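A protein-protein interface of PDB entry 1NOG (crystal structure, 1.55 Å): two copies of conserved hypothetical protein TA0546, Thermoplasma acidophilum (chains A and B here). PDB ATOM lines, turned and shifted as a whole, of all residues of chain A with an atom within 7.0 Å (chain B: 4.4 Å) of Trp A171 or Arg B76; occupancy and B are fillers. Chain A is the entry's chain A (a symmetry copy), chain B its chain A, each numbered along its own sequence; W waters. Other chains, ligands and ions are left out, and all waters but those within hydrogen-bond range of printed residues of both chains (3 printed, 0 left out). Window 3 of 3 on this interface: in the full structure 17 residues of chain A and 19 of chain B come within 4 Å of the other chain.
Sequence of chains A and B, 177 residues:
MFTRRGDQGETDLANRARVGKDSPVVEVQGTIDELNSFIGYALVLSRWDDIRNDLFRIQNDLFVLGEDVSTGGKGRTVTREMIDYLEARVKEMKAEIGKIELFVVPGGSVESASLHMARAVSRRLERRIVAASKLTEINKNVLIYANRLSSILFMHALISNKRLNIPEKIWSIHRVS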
ATOM      1  N   LEU A 102      24.564 -28.422   2.664  1.00  0.00           N
ATOM      2  CA  LEU A 102      25.355 -27.510   3.475  1.00  0.00           C
ATOM      3  C   LEU A 102      24.575 -26.935   4.647  1.00  0.00           C
ATOM      4  O   LEU A 102      23.356 -26.764   4.576  1.00  0.00           O
ATOM      5  CB  LEU A 102      25.894 -26.366   2.614  1.00  0.00           C
ATOM      6  CG  LEU A 102      26.869 -26.754   1.500  1.00  0.00           C
ATOM      7  CD1 LEU A 102      27.327 -25.500   0.771  1.00  0.00           C
ATOM      8  CD2 LEU A 102      28.064 -27.490   2.092  1.00  0.00           C
ATOM      9  N   PHE A 103      25.301 -26.644   5.724  1.00  0.00           N
ATOM     10  CA  PHE A 103      24.730 -26.073   6.935  1.00  0.00           C
ATOM     11  C   PHE A 103      24.071 -27.110   7.842  1.00  0.00           C
ATOM     12  O   PHE A 103      22.914 -26.968   8.234  1.00  0.00           O
ATOM     13  CB  PHE A 103      23.733 -24.967   6.570  1.00  0.00           C
ATOM     14  CG  PHE A 103      24.338 -23.858   5.750  1.00  0.00           C
ATOM     15  CD1 PHE A 103      23.562 -23.139   4.847  1.00  0.00           C
ATOM     16  CD2 PHE A 103      25.688 -23.534   5.879  1.00  0.00           C
ATOM     17  CE1 PHE A 103      24.120 -22.115   4.079  1.00  0.00           C
ATOM     18  CE2 PHE A 103      26.255 -22.512   5.118  1.00  0.00           C
ATOM     19  CZ  PHE A 103      25.468 -21.802   4.216  1.00  0.00           C
ATOM     20  N   VAL A 104      24.822 -28.156   8.169  1.00  0.00           N
ATOM     21  CA  VAL A 104      24.324 -29.194   9.060  1.00  0.00           C
ATOM     22  C   VAL A 104      24.381 -28.652  10.490  1.00  0.00           C
ATOM     23  O   VAL A 104      25.404 -28.109  10.909  1.00  0.00           O
ATOM     24  CB  VAL A 104      25.202 -30.470   8.981  1.00  0.00           C
ATOM     25  CG1 VAL A 104      24.801 -31.449  10.077  1.00  0.00           C
ATOM     26  CG2 VAL A 104      25.050 -31.121   7.616  1.00  0.00           C
ATOM     27  N   VAL A 105      23.278 -28.770  11.223  1.00  0.00           N
ATOM     28  CA  VAL A 105      23.240 -28.318  12.611  1.00  0.00           C
ATOM     29  C   VAL A 105      23.921 -29.442  13.392  1.00  0.00           C
ATOM     30  O   VAL A 105      23.445 -30.577  13.400  1.00  0.00           O
ATOM     31  CB  VAL A 105      21.788 -28.134  13.102  1.00  0.00           C
ATOM     32  CG1 VAL A 105      21.784 -27.664  14.552  1.00  0.00           C
ATOM     33  CG2 VAL A 105      21.061 -27.121  12.216  1.00  0.00           C
ATOM     34  N   LYS A 169      19.709 -32.272  10.772  1.00  0.00           N
ATOM     35  CA  LYS A 169      18.879 -31.079  10.745  1.00  0.00           C
ATOM     36  C   LYS A 169      19.719 -30.069   9.976  1.00  0.00           C
ATOM     37  O   LYS A 169      20.935 -29.994  10.159  1.00  0.00           O
ATOM     38  CB  LYS A 169      18.575 -30.601  12.164  1.00  0.00           C
ATOM     39  CG  LYS A 169      17.667 -31.564  12.915  1.00  0.00           C
ATOM     40  CD  LYS A 169      17.293 -31.058  14.293  1.00  0.00           C
ATOM     41  CE  LYS A 169      16.249 -31.960  14.934  1.00  0.00           C
ATOM     42  NZ  LYS A 169      15.034 -32.081  14.076  1.00  0.00           N
ATOM     43  N   ILE A 170      19.073 -29.316   9.094  1.00  0.00           N
ATOM     44  CA  ILE A 170      19.773 -28.347   8.262  1.00  0.00           C
ATOM     45  C   ILE A 170      19.303 -26.926   8.537  1.00  0.00           C
ATOM     46  O   ILE A 170      18.124 -26.695   8.800  1.00  0.00           O
ATOM     47  CB  ILE A 170      19.533 -28.646   6.762  1.00  0.00           C
ATOM     48  CG1 ILE A 170      19.853 -30.112   6.455  1.00  0.00           C
ATOM     49  CG2 ILE A 170      20.372 -27.713   5.904  1.00  0.00           C
ATOM     50  CD1 ILE A 170      21.292 -30.508   6.697  1.00  0.00           C
ATOM     51  N   TRP A 171      20.228 -25.974   8.476  1.00  0.00           N
ATOM     52  CA  TRP A 171      19.877 -24.576   8.693  1.00  0.00           C
ATOM     53  C   TRP A 171      19.419 -23.970   7.370  1.00  0.00           C
ATOM     54  O   TRP A 171      20.160 -23.984   6.386  1.00  0.00           O
ATOM     55  CB  TRP A 171      21.073 -23.789   9.222  1.00  0.00           C
ATOM     56  CG  TRP A 171      20.810 -22.311   9.313  1.00  0.00           C
ATOM     57  CD1 TRP A 171      19.887 -21.688  10.103  1.00  0.00           C
ATOM     58  CD2 TRP A 171      21.470 -21.276   8.574  1.00  0.00           C
ATOM     59  NE1 TRP A 171      19.931 -20.327   9.902  1.00  0.00           N
ATOM     60  CE2 TRP A 171      20.896 -20.048   8.969  1.00  0.00           C
ATOM     61  CE3 TRP A 171      22.495 -21.269   7.618  1.00  0.00           C
ATOM     62  CZ2 TRP A 171      21.312 -18.822   8.437  1.00  0.00           C
ATOM     63  CZ3 TRP A 171      22.910 -20.048   7.091  1.00  0.00           C
ATOM     64  CH2 TRP A 171      22.317 -18.842   7.504  1.00  0.00           C
ATOM     65  N   ASN B  60      20.360 -22.428  15.436  1.00  0.00           N
ATOM     66  CA  ASN B  60      20.021 -21.795  14.173  1.00  0.00           C
ATOM     67  C   ASN B  60      20.448 -20.329  14.216  1.00  0.00           C
ATOM     68  O   ASN B  60      20.973 -19.805  13.231  1.00  0.00           O
ATOM     69  CB  ASN B  60      18.525 -21.939  13.904  1.00  0.00           C
ATOM     70  CG  ASN B  60      18.162 -23.338  13.438  1.00  0.00           C
ATOM     71  OD1 ASN B  60      18.250 -23.649  12.253  1.00  0.00           O
ATOM     72  ND2 ASN B  60      17.781 -24.199  14.378  1.00  0.00           N
ATOM     73  N   PHE B  63      24.056 -19.605  13.199  1.00  0.00           N
ATOM     74  CA  PHE B  63      24.418 -19.550  11.786  1.00  0.00           C
ATOM     75  C   PHE B  63      24.196 -18.115  11.310  1.00  0.00           C
ATOM     76  O   PHE B  63      24.953 -17.595  10.487  1.00  0.00           O
ATOM     77  CB  PHE B  63      23.579 -20.524  10.957  1.00  0.00           C
ATOM     78  CG  PHE B  63      24.035 -21.951  11.056  1.00  0.00           C
ATOM     79  CD1 PHE B  63      23.431 -22.828  11.947  1.00  0.00           C
ATOM     80  CD2 PHE B  63      25.095 -22.407  10.280  1.00  0.00           C
ATOM     81  CE1 PHE B  63      23.878 -24.144  12.068  1.00  0.00           C
ATOM     82  CE2 PHE B  63      25.549 -23.719  10.392  1.00  0.00           C
ATOM     83  CZ  PHE B  63      24.939 -24.589  11.289  1.00  0.00           C
ATOM     84  N   VAL B  64      23.158 -17.472  11.841  1.00  0.00           N
ATOM     85  CA  VAL B  64      22.870 -16.085  11.484  1.00  0.00           C
ATOM     86  C   VAL B  64      23.963 -15.180  12.041  1.00  0.00           C
ATOM     87  O   VAL B  64      24.417 -14.250  11.371  1.00  0.00           O
ATOM     88  CB  VAL B  64      21.510 -15.627  12.054  1.00  0.00           C
ATOM     89  CG1 VAL B  64      21.325 -14.126  11.829  1.00  0.00           C
ATOM     90  CG2 VAL B  64      20.389 -16.405  11.391  1.00  0.00           C
ATOM     91  N   GLU B  67      26.983 -15.418   9.864  1.00  0.00           N
ATOM     92  CA  GLU B  67      26.832 -14.701   8.600  1.00  0.00           C
ATOM     93  C   GLU B  67      26.942 -13.197   8.821  1.00  0.00           C
ATOM     94  O   GLU B  67      27.552 -12.486   8.019  1.00  0.00           O
ATOM     95  CB  GLU B  67      25.488 -15.037   7.948  1.00  0.00           C
ATOM     96  CG  GLU B  67      25.282 -14.355   6.598  1.00  0.00           C
ATOM     97  CD  GLU B  67      24.054 -14.855   5.862  1.00  0.00           C
ATOM     98  OE1 GLU B  67      23.718 -14.278   4.806  1.00  0.00           O
ATOM     99  OE2 GLU B  67      23.428 -15.827   6.333  1.00  0.00           O
ATOM    100  N   ASP B  68      26.354 -12.715   9.911  1.00  0.00           N
ATOM    101  CA  ASP B  68      26.402 -11.295  10.245  1.00  0.00           C
ATOM    102  C   ASP B  68      27.871 -10.878  10.337  1.00  0.00           C
ATOM    103  O   ASP B  68      28.301  -9.908   9.710  1.00  0.00           O
ATOM    104  CB  ASP B  68      25.710 -11.052  11.593  1.00  0.00           C
ATOM    105  CG  ASP B  68      25.386  -9.585  11.836  1.00  0.00           C
ATOM    106  OD1 ASP B  68      26.140  -8.709  11.363  1.00  0.00           O
ATOM    107  OD2 ASP B  68      24.376  -9.310  12.519  1.00  0.00           O
ATOM    108  N   GLY B  75      24.832  -9.510   4.775  1.00  0.00           N
ATOM    109  CA  GLY B  75      23.880 -10.591   4.590  1.00  0.00           C
ATOM    110  C   GLY B  75      22.875 -10.605   5.726  1.00  0.00           C
ATOM    111  O   GLY B  75      22.458  -9.548   6.204  1.00  0.00           O
ATOM    112  N   ARG B  76      22.480 -11.796   6.162  1.00  0.00           N
ATOM    113  CA  ARG B  76      21.528 -11.907   7.261  1.00  0.00           C
ATOM    114  C   ARG B  76      22.181 -11.306   8.496  1.00  0.00           C
ATOM    115  O   ARG B  76      23.399 -11.372   8.655  1.00  0.00           O
ATOM    116  CB  ARG B  76      21.169 -13.372   7.511  1.00  0.00           C
ATOM    117  CG  ARG B  76      20.584 -14.067   6.292  1.00  0.00           C
ATOM    118  CD  ARG B  76      20.126 -15.479   6.608  1.00  0.00           C
ATOM    119  NE  ARG B  76      19.717 -16.194   5.401  1.00  0.00           N
ATOM    120  CZ  ARG B  76      19.162 -17.400   5.395  1.00  0.00           C
ATOM    121  NH1 ARG B  76      18.940 -18.039   6.536  1.00  0.00           N
ATOM    122  NH2 ARG B  76      18.827 -17.972   4.246  1.00  0.00           N
ATOM    123  N   THR B  77      21.375 -10.708   9.366  1.00  0.00           N
ATOM    124  CA  THR B  77      21.909 -10.092  10.571  1.00  0.00           C
ATOM    125  C   THR B  77      21.155 -10.515  11.818  1.00  0.00           C
ATOM    126  O   THR B  77      20.007 -10.953  11.747  1.00  0.00           O
ATOM    127  CB  THR B  77      21.854  -8.553  10.486  1.00  0.00           C
ATOM    128  OG1 THR B  77      20.520  -8.146  10.167  1.00  0.00           O
ATOM    129  CG2 THR B  77      22.810  -8.037   9.421  1.00  0.00           C
HETATM  130  O   HOH W   1      17.183 -25.901  11.267  1.00  0.00           O
HETATM  131  O   HOH W   2      17.120 -23.420   9.223  1.00  0.00           O
HETATM  132  O   HOH W   3      19.907 -21.069   4.963  1.00  0.00           O
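OE2 of Glu B67 lies within salt-bridge range of NE of Arg B76 (3.8 Å).
The backbone carbonyl oxygen of Arg B76 lies close to the backbone NH of Asp B68 (3.5 Å).
The backbone NH (N) of Trp A171 sits at hydrogen-bond distance from the backbone carbonyl oxygen (O) of Phe A103.
Among the printed residues, pairs that only touch across the chains: Trp A171 with Arg B76, Trp A171 with Phe B63, Trp A171 with Asn B60, Trp A171 with Glu B67, Val A104 with Phe B63 and Trp A171 with Val B64.
Trp A171 touches just these residues of chain B: Asn B60 (3.3 Å), Phe B63 (3.3 Å), Val B64 (3.9 Å), Glu B67 (3.4 Å) and Arg B76 (3.1 Å).
Of the printed residues of chain A, Arg B76 touches Trp A171 (3.1 Å).
Of the printed residues of chain B, Val A104 touches Phe B63 (3.6 Å).
Of the printed residues of chain A, Val B64 touches Trp A171 (3.9 Å).
Of the printed residues of chain A, Glu B67 touches Trp A171.
Ile A170 touches none of the printed residues of chain B.
Thr B77 touches none of the printed residues of chain A.
The nearest printed residue of chain B that does not touch Trp A171 is Asp B68 (7.7 Å).
The nearest printed residue of chain A that does not touch Glu B67 is Phe A103 (6.7 Å).
Hydrophobic or aromatic side chains of chain A that line the printed part of chain B: Trp A171.
Along chain A the printed residues that touch a printed residue of chain B span positions 104 to 171.
Printed residues of chain B that touch a printed residue of chain A: Asn B60, Phe B63, Val B64, Glu B67 and Arg B76.
Hydrophobic or aromatic side chains of chain B that line the printed part of chain A: Phe B63 and Val B64.
Among the printed residues, 6 pairs touch across the chains.
No position is printed for both chains.
Of the 6 pairs that touch across the chains among the printed residues, none has its exchanged pair printed and touching as well.
Water W1 lies within hydrogen-bond range of the side-chain amide oxygen (OD1) of Asn B60 (2.7 Å) and the backbone carbonyl oxygen (O) of Ile A170 (2.8 Å).
Water W2 lies within hydrogen-bond range of the side-chain amide oxygen (OD1) of Asn B60 and the backbone carbonyl oxygen (O) of Ile A170.
Water W3 bridges O of Trp A171 (3.3 Å) and NH2 of Arg B76 (3.4 Å).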
